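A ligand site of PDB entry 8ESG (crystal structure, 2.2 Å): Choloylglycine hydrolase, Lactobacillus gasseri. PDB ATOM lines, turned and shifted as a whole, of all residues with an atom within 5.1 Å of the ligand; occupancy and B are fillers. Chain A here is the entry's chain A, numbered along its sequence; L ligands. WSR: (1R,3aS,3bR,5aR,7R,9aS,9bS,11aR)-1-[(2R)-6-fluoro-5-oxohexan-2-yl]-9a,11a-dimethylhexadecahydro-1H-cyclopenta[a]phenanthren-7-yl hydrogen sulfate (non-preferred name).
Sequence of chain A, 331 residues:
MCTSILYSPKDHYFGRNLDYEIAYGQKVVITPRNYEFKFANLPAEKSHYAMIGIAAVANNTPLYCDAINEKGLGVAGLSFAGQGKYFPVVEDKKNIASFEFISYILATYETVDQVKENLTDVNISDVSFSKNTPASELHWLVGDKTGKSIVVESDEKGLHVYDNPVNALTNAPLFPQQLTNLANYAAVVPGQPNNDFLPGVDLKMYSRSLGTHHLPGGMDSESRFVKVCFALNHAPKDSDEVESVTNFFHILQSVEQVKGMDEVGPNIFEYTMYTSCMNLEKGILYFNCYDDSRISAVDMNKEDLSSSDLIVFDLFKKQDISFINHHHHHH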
ATOM      1  N   CYS A   2     -18.870  14.644  18.028  1.00  0.00           N
ATOM      2  CA  CYS A   2     -19.673  14.100  16.932  1.00  0.00           C
ATOM      3  C   CYS A   2     -20.454  15.203  16.239  1.00  0.00           C
ATOM      4  O   CYS A   2     -20.667  16.278  16.803  1.00  0.00           O
ATOM      5  CB  CYS A   2     -20.637  13.031  17.434  1.00  0.00           C
ATOM      6  SG  CYS A   2     -19.859  11.422  17.687  1.00  0.00           S
ATOM      7  N   ARG A  16     -24.186  11.184  10.306  1.00  0.00           N
ATOM      8  CA  ARG A  16     -23.390  11.756  11.373  1.00  0.00           C
ATOM      9  C   ARG A  16     -21.932  11.328  11.240  1.00  0.00           C
ATOM     10  O   ARG A  16     -21.614  10.306  10.629  1.00  0.00           O
ATOM     11  CB  ARG A  16     -23.920  11.355  12.762  1.00  0.00           C
ATOM     12  CG  ARG A  16     -24.059   9.848  12.963  1.00  0.00           C
ATOM     13  CD  ARG A  16     -22.816   9.235  13.621  1.00  0.00           C
ATOM     14  NE  ARG A  16     -22.538   9.803  14.934  1.00  0.00           N
ATOM     15  CZ  ARG A  16     -23.219   9.521  16.041  1.00  0.00           C
ATOM     16  NH1 ARG A  16     -24.223   8.669  16.031  1.00  0.00           N
ATOM     17  NH2 ARG A  16     -22.862  10.107  17.178  1.00  0.00           N
ATOM     18  N   ASN A  17     -21.058  12.132  11.839  1.00  0.00           N
ATOM     19  CA  ASN A  17     -19.694  11.729  12.147  1.00  0.00           C
ATOM     20  C   ASN A  17     -19.661  11.148  13.550  1.00  0.00           C
ATOM     21  O   ASN A  17     -20.294  11.672  14.466  1.00  0.00           O
ATOM     22  CB  ASN A  17     -18.733  12.922  12.073  1.00  0.00           C
ATOM     23  CG  ASN A  17     -18.218  13.169  10.675  1.00  0.00           C
ATOM     24  OD1 ASN A  17     -18.303  12.302   9.809  1.00  0.00           O
ATOM     25  ND2 ASN A  17     -17.661  14.350  10.450  1.00  0.00           N
ATOM     26  N   LEU A  18     -18.931  10.055  13.715  1.00  0.00           N
ATOM     27  CA  LEU A  18     -18.721   9.474  15.035  1.00  0.00           C
ATOM     28  C   LEU A  18     -17.248   9.680  15.397  1.00  0.00           C
ATOM     29  O   LEU A  18     -16.375   8.973  14.899  1.00  0.00           O
ATOM     30  CB  LEU A  18     -19.110   8.001  15.054  1.00  0.00           C
ATOM     31  CG  LEU A  18     -19.229   7.451  16.483  1.00  0.00           C
ATOM     32  CD1 LEU A  18     -20.610   6.864  16.733  1.00  0.00           C
ATOM     33  CD2 LEU A  18     -18.147   6.428  16.742  1.00  0.00           C
ATOM     34  N   ASP A  19     -17.005  10.661  16.255  1.00  0.00           N
ATOM     35  CA  ASP A  19     -15.648  11.032  16.666  1.00  0.00           C
ATOM     36  C   ASP A  19     -15.395  10.488  18.066  1.00  0.00           C
ATOM     37  O   ASP A  19     -15.943  11.004  19.043  1.00  0.00           O
ATOM     38  CB  ASP A  19     -15.470  12.553  16.637  1.00  0.00           C
ATOM     39  CG  ASP A  19     -15.963  13.173  15.335  1.00  0.00           C
ATOM     40  OD1 ASP A  19     -15.803  12.545  14.269  1.00  0.00           O
ATOM     41  OD2 ASP A  19     -16.506  14.295  15.381  1.00  0.00           O
ATOM     42  N   TYR A  20     -14.575   9.446  18.164  1.00  0.00           N
ATOM     43  CA  TYR A  20     -14.264   8.863  19.461  1.00  0.00           C
ATOM     44  C   TYR A  20     -12.857   8.289  19.425  1.00  0.00           C
ATOM     45  O   TYR A  20     -12.150   8.375  18.416  1.00  0.00           O
ATOM     46  CB  TYR A  20     -15.295   7.792  19.844  1.00  0.00           C
ATOM     47  CG  TYR A  20     -15.595   7.756  21.317  1.00  0.00           C
ATOM     48  CD1 TYR A  20     -15.936   8.914  22.009  1.00  0.00           C
ATOM     49  CD2 TYR A  20     -15.526   6.560  22.033  1.00  0.00           C
ATOM     50  CE1 TYR A  20     -16.200   8.882  23.363  1.00  0.00           C
ATOM     51  CE2 TYR A  20     -15.789   6.528  23.387  1.00  0.00           C
ATOM     52  CZ  TYR A  20     -16.132   7.692  24.043  1.00  0.00           C
ATOM     53  OH  TYR A  20     -16.395   7.659  25.398  1.00  0.00           O
ATOM     54  N   TYR A  24     -16.523   0.214  19.328  1.00  0.00           N
ATOM     55  CA  TYR A  24     -17.425  -0.628  20.105  1.00  0.00           C
ATOM     56  C   TYR A  24     -17.942  -1.817  19.312  1.00  0.00           C
ATOM     57  O   TYR A  24     -18.964  -2.414  19.667  1.00  0.00           O
ATOM     58  CB  TYR A  24     -18.603   0.211  20.626  1.00  0.00           C
ATOM     59  CG  TYR A  24     -18.276   1.020  21.856  1.00  0.00           C
ATOM     60  CD1 TYR A  24     -18.043   2.390  21.766  1.00  0.00           C
ATOM     61  CD2 TYR A  24     -18.220   0.430  23.111  1.00  0.00           C
ATOM     62  CE1 TYR A  24     -17.751   3.142  22.888  1.00  0.00           C
ATOM     63  CE2 TYR A  24     -17.928   1.183  24.233  1.00  0.00           C
ATOM     64  CZ  TYR A  24     -17.692   2.532  24.123  1.00  0.00           C
ATOM     65  OH  TYR A  24     -17.405   3.263  25.256  1.00  0.00           O
ATOM     66  N   GLN A  26     -18.978  -1.680  16.041  1.00  0.00           N
ATOM     67  CA  GLN A  26     -20.140  -1.206  15.312  1.00  0.00           C
ATOM     68  C   GLN A  26     -20.195  -1.825  13.925  1.00  0.00           C
ATOM     69  O   GLN A  26     -19.172  -2.140  13.312  1.00  0.00           O
ATOM     70  CB  GLN A  26     -20.110   0.318  15.198  1.00  0.00           C
ATOM     71  CG  GLN A  26     -20.326   1.036  16.526  1.00  0.00           C
ATOM     72  CD  GLN A  26     -19.029   1.554  17.124  1.00  0.00           C
ATOM     73  OE1 GLN A  26     -18.040   0.829  17.203  1.00  0.00           O
ATOM     74  NE2 GLN A  26     -19.033   2.809  17.541  1.00  0.00           N
ATOM     75  N   ALA A  56     -23.976  -1.498  17.328  1.00  0.00           N
ATOM     76  CA  ALA A  56     -23.118  -2.498  17.931  1.00  0.00           C
ATOM     77  C   ALA A  56     -23.981  -3.679  18.349  1.00  0.00           C
ATOM     78  O   ALA A  56     -24.855  -3.531  19.210  1.00  0.00           O
ATOM     79  CB  ALA A  56     -22.347  -1.923  19.122  1.00  0.00           C
ATOM     80  N   LEU A  63     -27.894  -2.221  19.257  1.00  0.00           N
ATOM     81  CA  LEU A  63     -27.774  -0.985  20.014  1.00  0.00           C
ATOM     82  C   LEU A  63     -27.331   0.100  19.036  1.00  0.00           C
ATOM     83  O   LEU A  63     -26.142   0.237  18.741  1.00  0.00           O
ATOM     84  CB  LEU A  63     -26.791  -1.142  21.172  1.00  0.00           C
ATOM     85  CG  LEU A  63     -27.285  -2.048  22.306  1.00  0.00           C
ATOM     86  CD1 LEU A  63     -26.159  -2.319  23.288  1.00  0.00           C
ATOM     87  CD2 LEU A  63     -28.473  -1.426  23.009  1.00  0.00           C
ATOM     88  N   TYR A  64     -28.301   0.857  18.536  1.00  0.00           N
ATOM     89  CA  TYR A  64     -28.071   1.752  17.413  1.00  0.00           C
ATOM     90  C   TYR A  64     -27.371   3.032  17.854  1.00  0.00           C
ATOM     91  O   TYR A  64     -27.619   3.559  18.946  1.00  0.00           O
ATOM     92  CB  TYR A  64     -29.391   2.106  16.729  1.00  0.00           C
ATOM     93  CG  TYR A  64     -29.792   1.144  15.628  1.00  0.00           C
ATOM     94  CD1 TYR A  64     -29.076   1.079  14.449  1.00  0.00           C
ATOM     95  CD2 TYR A  64     -30.895   0.317  15.778  1.00  0.00           C
ATOM     96  CE1 TYR A  64     -29.437   0.208  13.435  1.00  0.00           C
ATOM     97  CE2 TYR A  64     -31.265  -0.563  14.771  1.00  0.00           C
ATOM     98  CZ  TYR A  64     -30.539  -0.612  13.608  1.00  0.00           C
ATOM     99  OH  TYR A  64     -30.905  -1.483  12.602  1.00  0.00           O
ATOM    100  N   CYS A  65     -26.484   3.537  16.988  1.00  0.00           N
ATOM    101  CA  CYS A  65     -25.904   4.863  17.124  1.00  0.00           C
ATOM    102  C   CYS A  65     -26.621   5.899  16.277  1.00  0.00           C
ATOM    103  O   CYS A  65     -26.822   7.030  16.717  1.00  0.00           O
ATOM    104  CB  CYS A  65     -24.418   4.838  16.735  1.00  0.00           C
ATOM    105  SG  CYS A  65     -23.393   3.728  17.743  1.00  0.00           S
ATOM    106  N   GLY A  77     -27.834   9.473  17.785  1.00  0.00           N
ATOM    107  CA  GLY A  77     -27.462   9.705  19.165  1.00  0.00           C
ATOM    108  C   GLY A  77     -26.052  10.252  19.270  1.00  0.00           C
ATOM    109  O   GLY A  77     -25.113   9.719  18.670  1.00  0.00           O
ATOM    110  N   LEU A  78     -25.917  11.328  20.047  1.00  0.00           N
ATOM    111  CA  LEU A  78     -24.643  11.996  20.261  1.00  0.00           C
ATOM    112  C   LEU A  78     -24.419  12.170  21.755  1.00  0.00           C
ATOM    113  O   LEU A  78     -25.375  12.265  22.526  1.00  0.00           O
ATOM    114  CB  LEU A  78     -24.574  13.355  19.544  1.00  0.00           C
ATOM    115  CG  LEU A  78     -24.582  13.353  18.012  1.00  0.00           C
ATOM    116  CD1 LEU A  78     -26.002  13.262  17.463  1.00  0.00           C
ATOM    117  CD2 LEU A  78     -23.882  14.592  17.472  1.00  0.00           C
ATOM    118  N   SER A  79     -23.155  12.222  22.158  1.00  0.00           N
ATOM    119  CA  SER A  79     -22.833  12.339  23.575  1.00  0.00           C
ATOM    120  C   SER A  79     -23.248  13.699  24.106  1.00  0.00           C
ATOM    121  O   SER A  79     -23.174  14.719  23.416  1.00  0.00           O
ATOM    122  CB  SER A  79     -21.336  12.124  23.807  1.00  0.00           C
ATOM    123  OG  SER A  79     -20.888  12.861  24.928  1.00  0.00           O
ATOM    124  N   SER A  98     -32.252   5.008  27.598  1.00  0.00           N
ATOM    125  CA  SER A  98     -31.469   5.791  26.641  1.00  0.00           C
ATOM    126  C   SER A  98     -31.014   4.941  25.460  1.00  0.00           C
ATOM    127  O   SER A  98     -30.977   5.426  24.324  1.00  0.00           O
ATOM    128  CB  SER A  98     -30.262   6.414  27.341  1.00  0.00           C
ATOM    129  OG  SER A  98     -29.654   5.499  28.232  1.00  0.00           O
ATOM    130  N   PHE A  99     -30.676   3.671  25.700  1.00  0.00           N
ATOM    131  CA  PHE A  99     -30.154   2.834  24.626  1.00  0.00           C
ATOM    132  C   PHE A  99     -31.219   2.324  23.676  1.00  0.00           C
ATOM    133  O   PHE A  99     -30.894   1.945  22.549  1.00  0.00           O
ATOM    134  CB  PHE A  99     -29.370   1.649  25.211  1.00  0.00           C
ATOM    135  CG  PHE A  99     -30.180   0.775  26.124  1.00  0.00           C
ATOM    136  CD1 PHE A  99     -30.246   1.035  27.479  1.00  0.00           C
ATOM    137  CD2 PHE A  99     -30.863  -0.330  25.623  1.00  0.00           C
ATOM    138  CE1 PHE A  99     -30.987   0.220  28.324  1.00  0.00           C
ATOM    139  CE2 PHE A  99     -31.599  -1.146  26.459  1.00  0.00           C
ATOM    140  CZ  PHE A  99     -31.666  -0.864  27.812  1.00  0.00           C
ATOM    141  N   VAL A 127     -32.164   3.506  33.080  1.00  0.00           N
ATOM    142  CA  VAL A 127     -31.937   2.078  32.908  1.00  0.00           C
ATOM    143  C   VAL A 127     -30.764   1.898  31.944  1.00  0.00           C
ATOM    144  O   VAL A 127     -30.881   2.199  30.756  1.00  0.00           O
ATOM    145  CB  VAL A 127     -33.199   1.363  32.392  1.00  0.00           C
ATOM    146  CG1 VAL A 127     -32.895  -0.102  32.128  1.00  0.00           C
ATOM    147  CG2 VAL A 127     -34.339   1.506  33.377  1.00  0.00           C
ATOM    148  N   SER A 128     -29.649   1.396  32.463  1.00  0.00           N
ATOM    149  CA  SER A 128     -28.506   1.091  31.618  1.00  0.00           C
ATOM    150  C   SER A 128     -28.665  -0.302  31.012  1.00  0.00           C
ATOM    151  O   SER A 128     -29.547  -1.083  31.391  1.00  0.00           O
ATOM    152  CB  SER A 128     -27.205   1.179  32.422  1.00  0.00           C
ATOM    153  OG  SER A 128     -27.335   0.540  33.677  1.00  0.00           O
ATOM    154  N   PHE A 129     -27.811  -0.607  30.023  1.00  0.00           N
ATOM    155  CA  PHE A 129     -27.777  -1.963  29.480  1.00  0.00           C
ATOM    156  C   PHE A 129     -27.391  -2.955  30.573  1.00  0.00           C
ATOM    157  O   PHE A 129     -27.932  -4.066  30.640  1.00  0.00           O
ATOM    158  CB  PHE A 129     -26.799  -2.042  28.315  1.00  0.00           C
ATOM    159  N   LYS A 131     -24.273  -2.010  33.500  1.00  0.00           N
ATOM    160  CA  LYS A 131     -23.628  -1.130  34.470  1.00  0.00           C
ATOM    161  C   LYS A 131     -23.414   0.263  33.893  1.00  0.00           C
ATOM    162  O   LYS A 131     -22.758   0.426  32.860  1.00  0.00           O
ATOM    163  CB  LYS A 131     -22.301  -1.723  34.921  1.00  0.00           C
ATOM    164  N   LEU A 138     -26.512  11.049  26.724  1.00  0.00           N
ATOM    165  CA  LEU A 138     -26.688  11.225  25.291  1.00  0.00           C
ATOM    166  C   LEU A 138     -27.854  12.152  25.013  1.00  0.00           C
ATOM    167  O   LEU A 138     -28.796  12.250  25.804  1.00  0.00           O
ATOM    168  CB  LEU A 138     -26.922   9.885  24.580  1.00  0.00           C
ATOM    169  CG  LEU A 138     -25.819   8.822  24.692  1.00  0.00           C
ATOM    170  CD1 LEU A 138     -26.392   7.440  24.482  1.00  0.00           C
ATOM    171  CD2 LEU A 138     -24.704   9.099  23.696  1.00  0.00           C
ATOM    172  N   ASN A 171     -22.303  18.311  20.457  1.00  0.00           N
ATOM    173  CA  ASN A 171     -22.334  17.874  21.847  1.00  0.00           C
ATOM    174  C   ASN A 171     -22.736  19.009  22.784  1.00  0.00           C
ATOM    175  O   ASN A 171     -23.732  19.695  22.541  1.00  0.00           O
ATOM    176  CB  ASN A 171     -20.978  17.299  22.245  1.00  0.00           C
ATOM    177  CG  ASN A 171     -20.471  16.260  21.269  1.00  0.00           C
ATOM    178  OD1 ASN A 171     -19.508  16.502  20.536  1.00  0.00           O
ATOM    179  ND2 ASN A 171     -21.124  15.108  21.240  1.00  0.00           N
HETATM  180  C4  WSR L   1     -20.651   9.185  21.127  1.00  0.00           C
HETATM  181  C5  WSR L   1     -20.393   7.705  21.463  1.00  0.00           C
HETATM  182  C6  WSR L   1     -19.445   7.599  22.655  1.00  0.00           C
HETATM  183  C7  WSR L   1     -21.746   7.001  21.703  1.00  0.00           C
HETATM  184  C8  WSR L   1     -22.774   7.309  20.588  1.00  0.00           C
HETATM  185  C10 WSR L   1     -23.372   5.309  21.809  1.00  0.00           C
HETATM  186  C13 WSR L   1     -26.025   2.517  22.268  1.00  0.00           C
HETATM  187  C15 WSR L   1     -26.000   2.781  24.776  1.00  0.00           C
HETATM  188  C17 WSR L   1     -23.994   2.174  26.106  1.00  0.00           C
HETATM  189  C20 WSR L   1     -23.481   0.859  22.481  1.00  0.00           C
HETATM  190  C21 WSR L   1     -23.368   3.288  23.264  1.00  0.00           C
HETATM  191  C22 WSR L   1     -21.841   3.380  23.307  1.00  0.00           C
HETATM  192  C24 WSR L   1     -21.832   5.444  21.822  1.00  0.00           C
HETATM  193  C1  WSR L   1     -18.930  11.710  19.187  1.00  0.00           C
HETATM  194  C11 WSR L   1     -23.931   3.901  21.968  1.00  0.00           C
HETATM  195  C12 WSR L   1     -25.453   3.906  21.990  1.00  0.00           C
HETATM  196  C14 WSR L   1     -25.491   1.967  23.577  1.00  0.00           C
HETATM  197  C16 WSR L   1     -25.510   2.245  26.104  1.00  0.00           C
HETATM  198  C18 WSR L   1     -23.483   1.345  24.933  1.00  0.00           C
HETATM  199  C19 WSR L   1     -23.939   1.865  23.556  1.00  0.00           C
HETATM  200  C2  WSR L   1     -19.655  11.393  20.422  1.00  0.00           C
HETATM  201  C23 WSR L   1     -21.336   4.821  23.137  1.00  0.00           C
HETATM  202  C25 WSR L   1     -21.170   4.779  20.609  1.00  0.00           C
HETATM  203  C3  WSR L   1     -19.409  10.041  21.020  1.00  0.00           C
HETATM  204  C9  WSR L   1     -23.796   6.148  20.601  1.00  0.00           C
HETATM  205  O1  WSR L   1     -20.440  12.165  20.909  1.00  0.00           O
HETATM  206  O2  WSR L   1     -25.925   3.172  27.175  1.00  0.00           O
HETATM  207  O3  WSR L   1     -26.468   3.788  29.456  1.00  0.00           O
HETATM  208  O4  WSR L   1     -27.184   1.663  28.569  1.00  0.00           O
HETATM  209  O5  WSR L   1     -24.858   2.037  29.065  1.00  0.00           O
HETATM  210  S1  WSR L   1     -26.117   2.629  28.665  1.00  0.00           S
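The backbone NH (N) of Cys 2 sits at hydrogen-bond distance from the side-chain amide oxygen (OD1) of Asn 171 (3.2 Å). SG of Cys 2 lies within hydrogen-bond range of N of Asp 19. NH2 of Arg 16 is in hydrogen-bond range of SG of Cys 2, at 3.3 Å. The backbone carbonyl oxygen (O) of Ser 79 lies within hydrogen-bond range of the side-chain amide nitrogen (ND2) of Asn 171, at 3.0 Å. The guanidinium group (NH1) of Arg 16 is in hydrogen-bond range of the backbone carbonyl oxygen (O) of Cys 65, 3.1 Å away. The backbone carbonyl oxygen (O) of Gly 77 lies within hydrogen-bond range of the guanidinium group (NH2) of Arg 16, 2.7 Å away. The backbone carbonyl oxygen of Leu 63 is in hydrogen-bond range of the backbone NH of Ala 56, at 3.1 Å. The side-chain amide oxygen (OE1) of Gln 26 lies within hydrogen-bond range of the backbone NH (N) of Tyr 24 (2.7 Å).
The side-chain sulfur of Cys 2 is bonded to a carbon (C1) of the ligand (1.8 Å). N of Phe 129 sits at hydrogen-bond distance from O4 of the ligand (2.8 Å). The backbone NH (N) of Ser 79 lies within hydrogen-bond range of an oxygen (O1) of the ligand, 3.0 Å away. ND2 of Asn 171 sits at hydrogen-bond distance from O1 of the ligand.
O of Asp 19 touches C1 of the ligand, 3.1 Å away. CE1 of Tyr 20 touches C6 of the ligand (3.6 Å). CE1 of Tyr 24 touches C23 of the ligand, 3.97 Å away. Leu 63 touches the ligand. O of Tyr 64 touches C12 of the ligand (3.8 Å). Cys 65 touches the ligand. O of Gly 77 touches C8 of the ligand, at 3.9 Å. Ser 98 touches the ligand (OG to O3, 3.8 Å). CD1 of Phe 99 touches O4 of the ligand (3.3 Å). Ser 128 touches the ligand (CA to O4, 3.4 Å). Within 4 Å of the ligand: Cys 2, Asp 19, Tyr 20, Tyr 24, Leu 63, Tyr 64, Cys 65, Gly 77, Ser 79, Ser 98, Phe 99, Ser 128, Phe 129 and Asn 171. The nearest printed residue that does not touch the ligand is Leu 78 (4.1 Å).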
